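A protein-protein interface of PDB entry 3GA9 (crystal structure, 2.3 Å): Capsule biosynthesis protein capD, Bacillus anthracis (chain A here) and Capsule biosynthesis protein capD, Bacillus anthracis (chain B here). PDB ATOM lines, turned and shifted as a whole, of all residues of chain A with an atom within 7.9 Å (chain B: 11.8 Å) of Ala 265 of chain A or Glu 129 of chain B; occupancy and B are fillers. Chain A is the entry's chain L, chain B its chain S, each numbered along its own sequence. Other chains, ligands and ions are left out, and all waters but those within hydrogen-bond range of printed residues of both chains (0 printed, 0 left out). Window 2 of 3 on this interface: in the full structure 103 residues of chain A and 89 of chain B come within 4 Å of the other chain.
Of the 13 printed residues of chain A, 7 touch a printed residue of chain B.
Hydrophobic or aromatic side chains of chain A within 4 Å of the printed part of chain B: Ala 265, Tyr 267, Met 268 and Met 271.
Printed residues of chain B that touch a printed residue of chain A: Lys 92, Phe 109, Phe 111, Ala 116, Val 126, Glu 129, Leu 130, Lys 133 and Leu 135.
Ala 265 of chain A touches two residues of chain B.
Of chain A, only Ala 265 comes within 4 Å of Glu 129 of chain B.
Thr 264 of chain A touches just one residue of chain B: Val 126 (3.4 Å).
No residue of chain B comes within 4 Å of Thr 266 of chain A.
Of the printed residues of chain B, Ser 269 of chain A touches Lys 133 (3.3 Å).
Of the printed residues of chain A, Val 126 of chain B touches Thr 264 (3.4 Å).
Printed residues of chain A within 4 Å of Leu 130 of chain B: Ala 265.
The nearest residue of chain B that does not touch Ala 265 of chain A is Val 126 of chain B (4.2 Å).
The nearest residue of chain A that does not touch Glu 129 of chain B is Thr 266 of chain A (5.5 Å).
The side-chain amino group (NZ) of Lys 133 of chain B sits close to the side-chain hydroxyl (OG) of Ser 269 of chain A, 3.4 Å away.
Among the printed residues, pairs that only touch across the chains: Met 268 of chain A with Phe 111 of chain B (3.2 Å), Ala 265 of chain A with Leu 130 of chain B (3.3 Å), Glu 272 of chain A with Phe 111 of chain B (3.4 Å), Thr 264 of chain A with Val 126 of chain B (3.4 Å), Ala 265 of chain A with Glu 129 of chain B (3.6 Å), Met 268 of chain A with Phe 109 of chain B (3.7 Å), Tyr 267 of chain A with Lys 92 of chain B (3.9 Å), Met 268 of chain A with Ala 116 of chain B (3.9 Å), Met 271 of chain A with Phe 109 of chain B (3.9 Å) and Glu 272 of chain A with Leu 135 of chain B (3.9 Å).
The side-chain hydroxyl (OG) of Ser 123 of chain B is in hydrogen-bond range of the backbone NH (N) of Val 126 of chain B, 3.4 Å away.
The backbone NH of Leu 135 of chain B lies within hydrogen-bond range of the backbone carbonyl oxygen of Leu 130 of chain B (3.1 Å).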
ATOM      1  N   ASP A 260      19.222 -12.813 -20.009  1.00  0.00           N
ATOM      2  CA  ASP A 260      18.001 -12.180 -20.539  1.00  0.00           C
ATOM      3  C   ASP A 260      17.848 -10.725 -20.176  1.00  0.00           C
ATOM      4  O   ASP A 260      16.792 -10.133 -20.430  1.00  0.00           O
ATOM      5  CB  ASP A 260      16.768 -12.914 -20.057  1.00  0.00           C
ATOM      6  CG  ASP A 260      16.717 -14.318 -20.565  1.00  0.00           C
ATOM      7  OD1 ASP A 260      16.263 -15.201 -19.803  1.00  0.00           O
ATOM      8  OD2 ASP A 260      17.153 -14.534 -21.723  1.00  0.00           O
ATOM      9  N   VAL A 261      18.915 -10.166 -19.600  1.00  0.00           N
ATOM     10  CA  VAL A 261      18.916  -8.813 -19.037  1.00  0.00           C
ATOM     11  C   VAL A 261      18.545  -7.755 -20.073  1.00  0.00           C
ATOM     12  O   VAL A 261      17.791  -6.832 -19.765  1.00  0.00           O
ATOM     13  CB  VAL A 261      20.262  -8.487 -18.296  1.00  0.00           C
ATOM     14  CG1 VAL A 261      21.444  -8.392 -19.261  1.00  0.00           C
ATOM     15  CG2 VAL A 261      20.131  -7.227 -17.444  1.00  0.00           C
ATOM     16  N   ASP A 262      19.023  -7.941 -21.309  1.00  0.00           N
ATOM     17  CA  ASP A 262      18.737  -7.024 -22.424  1.00  0.00           C
ATOM     18  C   ASP A 262      17.333  -7.165 -23.026  1.00  0.00           C
ATOM     19  O   ASP A 262      16.911  -6.301 -23.791  1.00  0.00           O
ATOM     20  CB  ASP A 262      19.806  -7.149 -23.526  1.00  0.00           C
ATOM     21  CG  ASP A 262      21.230  -6.824 -23.024  1.00  0.00           C
ATOM     22  OD1 ASP A 262      21.400  -5.856 -22.244  1.00  0.00           O
ATOM     23  OD2 ASP A 262      22.183  -7.534 -23.428  1.00  0.00           O
ATOM     24  N   HIS A 263      16.616  -8.240 -22.689  1.00  0.00           N
ATOM     25  CA  HIS A 263      15.238  -8.420 -23.153  1.00  0.00           C
ATOM     26  C   HIS A 263      14.333  -8.216 -21.963  1.00  0.00           C
ATOM     27  O   HIS A 263      14.187  -9.107 -21.122  1.00  0.00           O
ATOM     28  CB  HIS A 263      15.010  -9.814 -23.767  1.00  0.00           C
ATOM     29  CG  HIS A 263      16.177 -10.332 -24.556  1.00  0.00           C
ATOM     30  ND1 HIS A 263      16.337 -10.092 -25.906  1.00  0.00           N
ATOM     31  CD2 HIS A 263      17.244 -11.083 -24.182  1.00  0.00           C
ATOM     32  CE1 HIS A 263      17.452 -10.666 -26.329  1.00  0.00           C
ATOM     33  NE2 HIS A 263      18.021 -11.275 -25.302  1.00  0.00           N
ATOM     34  N   THR A 264      13.726  -7.041 -21.889  1.00  0.00           N
ATOM     35  CA  THR A 264      13.013  -6.645 -20.687  1.00  0.00           C
ATOM     36  C   THR A 264      11.954  -7.632 -20.219  1.00  0.00           C
ATOM     37  O   THR A 264      11.946  -7.995 -19.031  1.00  0.00           O
ATOM     38  CB  THR A 264      12.476  -5.205 -20.764  1.00  0.00           C
ATOM     39  OG1 THR A 264      13.434  -4.350 -20.148  1.00  0.00           O
ATOM     40  CG2 THR A 264      11.151  -5.047 -20.024  1.00  0.00           C
ATOM     41  N   ALA A 265      11.088  -8.075 -21.129  1.00  0.00           N
ATOM     42  CA  ALA A 265       9.963  -8.940 -20.737  1.00  0.00           C
ATOM     43  C   ALA A 265      10.426 -10.308 -20.225  1.00  0.00           C
ATOM     44  O   ALA A 265       9.847 -10.842 -19.278  1.00  0.00           O
ATOM     45  CB  ALA A 265       8.978  -9.098 -21.863  1.00  0.00           C
ATOM     46  N   THR A 266      11.474 -10.853 -20.849  1.00  0.00           N
ATOM     47  CA  THR A 266      12.094 -12.094 -20.380  1.00  0.00           C
ATOM     48  C   THR A 266      12.662 -11.885 -18.972  1.00  0.00           C
ATOM     49  O   THR A 266      12.289 -12.614 -18.027  1.00  0.00           O
ATOM     50  CB  THR A 266      13.237 -12.595 -21.299  1.00  0.00           C
ATOM     51  OG1 THR A 266      12.910 -12.378 -22.683  1.00  0.00           O
ATOM     52  CG2 THR A 266      13.486 -14.082 -21.055  1.00  0.00           C
ATOM     53  N   TYR A 267      13.542 -10.881 -18.836  1.00  0.00           N
ATOM     54  CA  TYR A 267      14.193 -10.593 -17.557  1.00  0.00           C
ATOM     55  C   TYR A 267      13.143 -10.508 -16.499  1.00  0.00           C
ATOM     56  O   TYR A 267      13.204 -11.261 -15.528  1.00  0.00           O
ATOM     57  CB  TYR A 267      15.014  -9.305 -17.573  1.00  0.00           C
ATOM     58  CG  TYR A 267      16.034  -9.241 -16.441  1.00  0.00           C
ATOM     59  CD1 TYR A 267      17.104 -10.145 -16.384  1.00  0.00           C
ATOM     60  CD2 TYR A 267      15.936  -8.283 -15.432  1.00  0.00           C
ATOM     61  CE1 TYR A 267      18.054 -10.084 -15.355  1.00  0.00           C
ATOM     62  CE2 TYR A 267      16.888  -8.217 -14.394  1.00  0.00           C
ATOM     63  CZ  TYR A 267      17.934  -9.117 -14.365  1.00  0.00           C
ATOM     64  OH  TYR A 267      18.874  -9.062 -13.358  1.00  0.00           O
ATOM     65  N   MET A 268      12.160  -9.635 -16.722  1.00  0.00           N
ATOM     66  CA  MET A 268      11.085  -9.439 -15.772  1.00  0.00           C
ATOM     67  C   MET A 268      10.350 -10.713 -15.516  1.00  0.00           C
ATOM     68  O   MET A 268      10.061 -11.044 -14.360  1.00  0.00           O
ATOM     69  CB  MET A 268      10.121  -8.362 -16.225  1.00  0.00           C
ATOM     70  CG  MET A 268      10.631  -7.007 -15.850  1.00  0.00           C
ATOM     71  SD  MET A 268       9.617  -5.617 -16.636  1.00  0.00           S
ATOM     72  CE  MET A 268       8.062  -5.668 -15.536  1.00  0.00           C
ATOM     73  N   SER A 269      10.082 -11.447 -16.591  1.00  0.00           N
ATOM     74  CA  SER A 269       9.258 -12.657 -16.516  1.00  0.00           C
ATOM     75  C   SER A 269       9.857 -13.671 -15.556  1.00  0.00           C
ATOM     76  O   SER A 269       9.165 -14.198 -14.691  1.00  0.00           O
ATOM     77  CB  SER A 269       9.087 -13.257 -17.919  1.00  0.00           C
ATOM     78  OG  SER A 269       8.354 -14.465 -17.882  1.00  0.00           O
ATOM     79  N   LYS A 270      11.149 -13.915 -15.705  1.00  0.00           N
ATOM     80  CA  LYS A 270      11.860 -14.855 -14.870  1.00  0.00           C
ATOM     81  C   LYS A 270      12.026 -14.413 -13.409  1.00  0.00           C
ATOM     82  O   LYS A 270      11.903 -15.245 -12.508  1.00  0.00           O
ATOM     83  CB  LYS A 270      13.212 -15.177 -15.484  1.00  0.00           C
ATOM     84  CG  LYS A 270      13.125 -15.600 -16.932  1.00  0.00           C
ATOM     85  CD  LYS A 270      14.462 -16.134 -17.395  1.00  0.00           C
ATOM     86  CE  LYS A 270      14.307 -17.087 -18.562  1.00  0.00           C
ATOM     87  NZ  LYS A 270      15.665 -17.612 -18.863  1.00  0.00           N
ATOM     88  N   MET A 271      12.311 -13.127 -13.173  1.00  0.00           N
ATOM     89  CA  MET A 271      12.304 -12.536 -11.811  1.00  0.00           C
ATOM     90  C   MET A 271      10.981 -12.762 -11.073  1.00  0.00           C
ATOM     91  O   MET A 271      10.957 -13.155  -9.906  1.00  0.00           O
ATOM     92  CB  MET A 271      12.624 -11.034 -11.853  1.00  0.00           C
ATOM     93  CG  MET A 271      14.085 -10.742 -12.154  1.00  0.00           C
ATOM     94  SD  MET A 271      15.320 -11.699 -10.930  1.00  0.00           S
ATOM     95  CE  MET A 271      17.011 -11.321 -11.856  1.00  0.00           C
ATOM     96  N   GLU A 272       9.891 -12.511 -11.784  1.00  0.00           N
ATOM     97  CA  GLU A 272       8.562 -12.795 -11.315  1.00  0.00           C
ATOM     98  C   GLU A 272       8.421 -14.245 -10.876  1.00  0.00           C
ATOM     99  O   GLU A 272       7.721 -14.533  -9.911  1.00  0.00           O
ATOM    100  CB  GLU A 272       7.565 -12.414 -12.411  1.00  0.00           C
ATOM    101  CG  GLU A 272       6.508 -13.446 -12.772  1.00  0.00           C
ATOM    102  CD  GLU A 272       5.477 -13.660 -11.677  1.00  0.00           C
ATOM    103  OE1 GLU A 272       5.379 -12.806 -10.782  1.00  0.00           O
ATOM    104  OE2 GLU A 272       4.774 -14.691 -11.701  1.00  0.00           O
ATOM    105  N   LYS B  92      22.827  -8.280 -11.593  1.00  0.00           N
ATOM    106  CA  LYS B  92      23.562  -7.412 -12.517  1.00  0.00           C
ATOM    107  C   LYS B  92      24.979  -7.177 -12.031  1.00  0.00           C
ATOM    108  O   LYS B  92      25.924  -7.307 -12.797  1.00  0.00           O
ATOM    109  CB  LYS B  92      22.847  -6.080 -12.717  1.00  0.00           C
ATOM    110  CG  LYS B  92      21.491  -6.225 -13.309  1.00  0.00           C
ATOM    111  CD  LYS B  92      20.722  -4.921 -13.370  1.00  0.00           C
ATOM    112  CE  LYS B  92      19.265  -5.212 -13.556  1.00  0.00           C
ATOM    113  NZ  LYS B  92      18.443  -3.994 -13.654  1.00  0.00           N
ATOM    114  N   PHE B 109      11.330  -2.657 -10.922  1.00  0.00           N
ATOM    115  CA  PHE B 109       9.987  -3.234 -11.041  1.00  0.00           C
ATOM    116  C   PHE B 109       9.823  -4.212  -9.894  1.00  0.00           C
ATOM    117  O   PHE B 109      10.770  -4.838  -9.490  1.00  0.00           O
ATOM    118  CB  PHE B 109       9.822  -3.969 -12.409  1.00  0.00           C
ATOM    119  CG  PHE B 109      10.873  -5.015 -12.640  1.00  0.00           C
ATOM    120  CD1 PHE B 109      12.074  -4.684 -13.253  1.00  0.00           C
ATOM    121  CD2 PHE B 109      10.700  -6.307 -12.164  1.00  0.00           C
ATOM    122  CE1 PHE B 109      13.086  -5.634 -13.401  1.00  0.00           C
ATOM    123  CE2 PHE B 109      11.699  -7.259 -12.318  1.00  0.00           C
ATOM    124  CZ  PHE B 109      12.897  -6.915 -12.930  1.00  0.00           C
ATOM    125  N   PHE B 111       6.717  -7.255  -8.312  1.00  0.00           N
ATOM    126  CA  PHE B 111       5.469  -7.954  -8.619  1.00  0.00           C
ATOM    127  C   PHE B 111       4.609  -8.167  -7.378  1.00  0.00           C
ATOM    128  O   PHE B 111       5.128  -8.488  -6.324  1.00  0.00           O
ATOM    129  CB  PHE B 111       5.790  -9.282  -9.298  1.00  0.00           C
ATOM    130  CG  PHE B 111       6.702  -9.143 -10.490  1.00  0.00           C
ATOM    131  CD1 PHE B 111       8.076  -9.353 -10.362  1.00  0.00           C
ATOM    132  CD2 PHE B 111       6.191  -8.800 -11.732  1.00  0.00           C
ATOM    133  CE1 PHE B 111       8.937  -9.235 -11.468  1.00  0.00           C
ATOM    134  CE2 PHE B 111       7.036  -8.672 -12.846  1.00  0.00           C
ATOM    135  CZ  PHE B 111       8.414  -8.890 -12.716  1.00  0.00           C
ATOM    136  N   ASN B 114       0.544 -11.150 -10.009  1.00  0.00           N
ATOM    137  CA  ASN B 114       0.052 -10.856 -11.364  1.00  0.00           C
ATOM    138  C   ASN B 114      -0.079  -9.377 -11.740  1.00  0.00           C
ATOM    139  O   ASN B 114      -0.580  -9.066 -12.826  1.00  0.00           O
ATOM    140  CB  ASN B 114      -1.269 -11.604 -11.666  1.00  0.00           C
ATOM    141  CG  ASN B 114      -1.078 -13.125 -11.772  1.00  0.00           C
ATOM    142  OD1 ASN B 114      -2.040 -13.896 -11.649  1.00  0.00           O
ATOM    143  ND2 ASN B 114       0.169 -13.558 -12.011  1.00  0.00           N
ATOM    144  N   ALA B 116       2.681  -6.431 -12.285  1.00  0.00           N
ATOM    145  CA  ALA B 116       4.058  -5.956 -12.288  1.00  0.00           C
ATOM    146  C   ALA B 116       4.042  -4.437 -12.063  1.00  0.00           C
ATOM    147  O   ALA B 116       3.424  -3.728 -12.845  1.00  0.00           O
ATOM    148  CB  ALA B 116       4.725  -6.288 -13.605  1.00  0.00           C
ATOM    149  N   THR B 118       6.035  -0.880 -12.125  1.00  0.00           N
ATOM    150  CA  THR B 118       7.226  -0.316 -12.792  1.00  0.00           C
ATOM    151  C   THR B 118       7.566   1.094 -12.360  1.00  0.00           C
ATOM    152  O   THR B 118       6.689   1.925 -12.130  1.00  0.00           O
ATOM    153  CB  THR B 118       7.051  -0.204 -14.306  1.00  0.00           C
ATOM    154  OG1 THR B 118       5.969  -1.032 -14.727  1.00  0.00           O
ATOM    155  CG2 THR B 118       8.347  -0.601 -15.028  1.00  0.00           C
ATOM    156  N   ILE B 120       9.582   3.146 -14.309  1.00  0.00           N
ATOM    157  CA  ILE B 120       9.485   3.902 -15.568  1.00  0.00           C
ATOM    158  C   ILE B 120       8.510   3.213 -16.543  1.00  0.00           C
ATOM    159  O   ILE B 120       8.478   1.984 -16.640  1.00  0.00           O
ATOM    160  CB  ILE B 120      10.925   4.144 -16.195  1.00  0.00           C
ATOM    161  CG1 ILE B 120      11.154   5.627 -16.591  1.00  0.00           C
ATOM    162  CG2 ILE B 120      11.313   3.082 -17.254  1.00  0.00           C
ATOM    163  CD1 ILE B 120      10.223   6.209 -17.693  1.00  0.00           C
ATOM    164  N   GLN B 121       7.705   3.999 -17.244  1.00  0.00           N
ATOM    165  CA  GLN B 121       6.713   3.436 -18.155  1.00  0.00           C
ATOM    166  C   GLN B 121       7.347   2.713 -19.357  1.00  0.00           C
ATOM    167  O   GLN B 121       8.297   3.214 -19.957  1.00  0.00           O
ATOM    168  CB  GLN B 121       5.780   4.525 -18.630  1.00  0.00           C
ATOM    169  CG  GLN B 121       4.582   4.024 -19.381  1.00  0.00           C
ATOM    170  CD  GLN B 121       3.710   5.164 -19.827  1.00  0.00           C
ATOM    171  OE1 GLN B 121       4.085   6.329 -19.709  1.00  0.00           O
ATOM    172  NE2 GLN B 121       2.536   4.841 -20.344  1.00  0.00           N
ATOM    173  N   LEU B 122       6.807   1.538 -19.695  1.00  0.00           N
ATOM    174  CA  LEU B 122       7.406   0.661 -20.716  1.00  0.00           C
ATOM    175  C   LEU B 122       6.680   0.631 -22.078  1.00  0.00           C
ATOM    176  O   LEU B 122       5.513   1.019 -22.193  1.00  0.00           O
ATOM    177  CB  LEU B 122       7.486  -0.762 -20.183  1.00  0.00           C
ATOM    178  CG  LEU B 122       8.011  -1.061 -18.787  1.00  0.00           C
ATOM    179  CD1 LEU B 122       7.241  -2.271 -18.253  1.00  0.00           C
ATOM    180  CD2 LEU B 122       9.526  -1.286 -18.811  1.00  0.00           C
ATOM    181  N   SER B 123       7.379   0.139 -23.096  1.00  0.00           N
ATOM    182  CA  SER B 123       6.820   0.031 -24.455  1.00  0.00           C
ATOM    183  C   SER B 123       5.697  -0.999 -24.602  1.00  0.00           C
ATOM    184  O   SER B 123       5.570  -1.931 -23.791  1.00  0.00           O
ATOM    185  CB  SER B 123       7.928  -0.292 -25.468  1.00  0.00           C
ATOM    186  OG  SER B 123       8.281  -1.667 -25.446  1.00  0.00           O
ATOM    187  N   SER B 124       4.902  -0.815 -25.658  1.00  0.00           N
ATOM    188  CA  SER B 124       3.883  -1.782 -26.107  1.00  0.00           C
ATOM    189  C   SER B 124       4.462  -3.190 -26.306  1.00  0.00           C
ATOM    190  O   SER B 124       3.954  -4.169 -25.744  1.00  0.00           O
ATOM    191  CB  SER B 124       3.260  -1.302 -27.420  1.00  0.00           C
ATOM    192  OG  SER B 124       4.252  -1.212 -28.430  1.00  0.00           O
ATOM    193  N   GLU B 125       5.526  -3.271 -27.109  1.00  0.00           N
ATOM    194  CA  GLU B 125       6.251  -4.520 -27.313  1.00  0.00           C
ATOM    195  C   GLU B 125       6.279  -5.286 -25.979  1.00  0.00           C
ATOM    196  O   GLU B 125       5.611  -6.329 -25.847  1.00  0.00           O
ATOM    197  CB  GLU B 125       7.656  -4.258 -27.909  1.00  0.00           C
ATOM    198  CG  GLU B 125       8.724  -5.382 -27.701  1.00  0.00           C
ATOM    199  CD  GLU B 125       8.823  -6.435 -28.840  1.00  0.00           C
ATOM    200  OE1 GLU B 125       7.795  -6.780 -29.477  1.00  0.00           O
ATOM    201  OE2 GLU B 125       9.949  -6.938 -29.084  1.00  0.00           O
ATOM    202  N   VAL B 126       6.988  -4.737 -25.007  1.00  0.00           N
ATOM    203  CA  VAL B 126       7.131  -5.360 -23.701  1.00  0.00           C
ATOM    204  C   VAL B 126       5.828  -5.597 -22.948  1.00  0.00           C
ATOM    205  O   VAL B 126       5.618  -6.659 -22.414  1.00  0.00           O
ATOM    206  CB  VAL B 126       8.104  -4.569 -22.833  1.00  0.00           C
ATOM    207  CG1 VAL B 126       8.019  -5.035 -21.446  1.00  0.00           C
ATOM    208  CG2 VAL B 126       9.509  -4.747 -23.339  1.00  0.00           C
ATOM    209  N   LYS B 127       4.961  -4.610 -22.911  1.00  0.00           N
ATOM    210  CA  LYS B 127       3.659  -4.720 -22.215  1.00  0.00           C
ATOM    211  C   LYS B 127       2.759  -5.864 -22.699  1.00  0.00           C
ATOM    212  O   LYS B 127       1.987  -6.434 -21.923  1.00  0.00           O
ATOM    213  CB  LYS B 127       2.901  -3.400 -22.265  1.00  0.00           C
ATOM    214  CG  LYS B 127       3.365  -2.450 -21.199  1.00  0.00           C
ATOM    215  CD  LYS B 127       2.890  -1.032 -21.390  1.00  0.00           C
ATOM    216  CE  LYS B 127       3.555  -0.147 -20.319  1.00  0.00           C
ATOM    217  NZ  LYS B 127       3.145   1.285 -20.351  1.00  0.00           N
ATOM    218  N   ASN B 128       2.874  -6.183 -23.986  1.00  0.00           N
ATOM    219  CA  ASN B 128       2.159  -7.298 -24.586  1.00  0.00           C
ATOM    220  C   ASN B 128       2.756  -8.635 -24.166  1.00  0.00           C
ATOM    221  O   ASN B 128       2.031  -9.520 -23.701  1.00  0.00           O
ATOM    222  CB  ASN B 128       2.164  -7.169 -26.114  1.00  0.00           C
ATOM    223  CG  ASN B 128       1.318  -6.012 -26.607  1.00  0.00           C
ATOM    224  OD1 ASN B 128       0.438  -5.515 -25.895  1.00  0.00           O
ATOM    225  ND2 ASN B 128       1.569  -5.584 -27.836  1.00  0.00           N
ATOM    226  N   GLU B 129       4.076  -8.772 -24.324  1.00  0.00           N
ATOM    227  CA  GLU B 129       4.790  -9.998 -23.957  1.00  0.00           C
ATOM    228  C   GLU B 129       4.515 -10.423 -22.521  1.00  0.00           C
ATOM    229  O   GLU B 129       4.465 -11.620 -22.222  1.00  0.00           O
ATOM    230  CB  GLU B 129       6.292  -9.831 -24.133  1.00  0.00           C
ATOM    231  CG  GLU B 129       6.744  -9.552 -25.547  1.00  0.00           C
ATOM    232  CD  GLU B 129       8.228  -9.240 -25.625  1.00  0.00           C
ATOM    233  OE1 GLU B 129       8.609  -8.049 -25.476  1.00  0.00           O
ATOM    234  OE2 GLU B 129       9.015 -10.195 -25.843  1.00  0.00           O
ATOM    235  N   LEU B 130       4.345  -9.435 -21.643  1.00  0.00           N
ATOM    236  CA  LEU B 130       4.086  -9.675 -20.229  1.00  0.00           C
ATOM    237  C   LEU B 130       2.600  -9.882 -19.954  1.00  0.00           C
ATOM    238  O   LEU B 130       2.229 -10.605 -19.014  1.00  0.00           O
ATOM    239  CB  LEU B 130       4.653  -8.539 -19.374  1.00  0.00           C
ATOM    240  CG  LEU B 130       6.176  -8.376 -19.459  1.00  0.00           C
ATOM    241  CD1 LEU B 130       6.574  -6.986 -19.027  1.00  0.00           C
ATOM    242  CD2 LEU B 130       6.930  -9.430 -18.646  1.00  0.00           C
ATOM    243  N   SER B 131       1.759  -9.247 -20.776  1.00  0.00           N
ATOM    244  CA  SER B 131       0.313  -9.490 -20.750  1.00  0.00           C
ATOM    245  C   SER B 131       0.031 -10.963 -21.095  1.00  0.00           C
ATOM    246  O   SER B 131      -0.832 -11.613 -20.481  1.00  0.00           O
ATOM    247  CB  SER B 131      -0.404  -8.552 -21.719  1.00  0.00           C
ATOM    248  OG  SER B 131      -1.600  -8.062 -21.138  1.00  0.00           O
ATOM    249  N   ARG B 132       0.806 -11.481 -22.052  1.00  0.00           N
ATOM    250  CA  ARG B 132       0.757 -12.892 -22.446  1.00  0.00           C
ATOM    251  C   ARG B 132       1.077 -13.901 -21.358  1.00  0.00           C
ATOM    252  O   ARG B 132       0.713 -15.066 -21.488  1.00  0.00           O
ATOM    253  CB  ARG B 132       1.646 -13.170 -23.658  1.00  0.00           C
ATOM    254  CG  ARG B 132       0.851 -13.230 -24.933  1.00  0.00           C
ATOM    255  CD  ARG B 132       1.485 -14.112 -25.992  1.00  0.00           C
ATOM    256  NE  ARG B 132       0.857 -13.806 -27.274  1.00  0.00           N
ATOM    257  CZ  ARG B 132       1.381 -12.996 -28.188  1.00  0.00           C
ATOM    258  NH1 ARG B 132       0.714 -12.759 -29.316  1.00  0.00           N
ATOM    259  NH2 ARG B 132       2.574 -12.435 -27.978  1.00  0.00           N
ATOM    260  N   LYS B 133       1.763 -13.479 -20.301  1.00  0.00           N
ATOM    261  CA  LYS B 133       2.077 -14.407 -19.217  1.00  0.00           C
ATOM    262  C   LYS B 133       1.162 -14.208 -18.003  1.00  0.00           C
ATOM    263  O   LYS B 133       1.413 -14.736 -16.922  1.00  0.00           O
ATOM    264  CB  LYS B 133       3.565 -14.369 -18.866  1.00  0.00           C
ATOM    265  CG  LYS B 133       4.455 -14.696 -20.043  1.00  0.00           C
ATOM    266  CD  LYS B 133       5.716 -15.375 -19.580  1.00  0.00           C
ATOM    267  CE  LYS B 133       6.765 -15.415 -20.677  1.00  0.00           C
ATOM    268  NZ  LYS B 133       7.276 -14.063 -21.042  1.00  0.00           N
ATOM    269  N   GLY B 134       0.074 -13.473 -18.206  1.00  0.00           N
ATOM    270  CA  GLY B 134      -0.909 -13.267 -17.160  1.00  0.00           C
ATOM    271  C   GLY B 134      -0.593 -12.101 -16.244  1.00  0.00           C
ATOM    272  O   GLY B 134      -1.326 -11.873 -15.276  1.00  0.00           O
ATOM    273  N   LEU B 135       0.428 -11.329 -16.596  1.00  0.00           N
ATOM    274  CA  LEU B 135       0.824 -10.148 -15.820  1.00  0.00           C
ATOM    275  C   LEU B 135       0.338  -8.799 -16.373  1.00  0.00           C
ATOM    276  O   LEU B 135       0.431  -8.539 -17.556  1.00  0.00           O
ATOM    277  CB  LEU B 135       2.340 -10.118 -15.698  1.00  0.00           C
ATOM    278  CG  LEU B 135       2.962 -11.342 -15.071  1.00  0.00           C
ATOM    279  CD1 LEU B 135       4.422 -11.331 -15.331  1.00  0.00           C
ATOM    280  CD2 LEU B 135       2.679 -11.352 -13.605  1.00  0.00           C
ATOM    281  N   ASN B 136      -0.139  -7.922 -15.506  1.00  0.00           N
ATOM    282  CA  ASN B 136      -0.573  -6.608 -15.988  1.00  0.00           C
ATOM    283  C   ASN B 136       0.206  -5.402 -15.446  1.00  0.00           C
ATOM    284  O   ASN B 136      -0.098  -4.856 -14.379  1.00  0.00           O
ATOM    285  CB  ASN B 136      -2.086  -6.427 -15.832  1.00  0.00           C
ATOM    286  CG  ASN B 136      -2.556  -6.670 -14.421  1.00  0.00           C
ATOM    287  OD1 ASN B 136      -1.768  -6.621 -13.481  1.00  0.00           O
ATOM    288  ND2 ASN B 136      -3.855  -6.926 -14.257  1.00  0.00           N
ATOM    289  N   VAL B 137       1.204  -4.989 -16.222  1.00  0.00           N
ATOM    290  CA  VAL B 137       2.062  -3.845 -15.909  1.00  0.00           C
ATOM    291  C   VAL B 137       1.304  -2.635 -15.341  1.00  0.00           C
ATOM    292  O   VAL B 137       0.271  -2.231 -15.859  1.00  0.00           O
ATOM    293  CB  VAL B 137       2.938  -3.450 -17.142  1.00  0.00           C
ATOM    294  CG1 VAL B 137       3.624  -2.080 -16.959  1.00  0.00           C
ATOM    295  CG2 VAL B 137       3.977  -4.538 -17.443  1.00  0.00           C
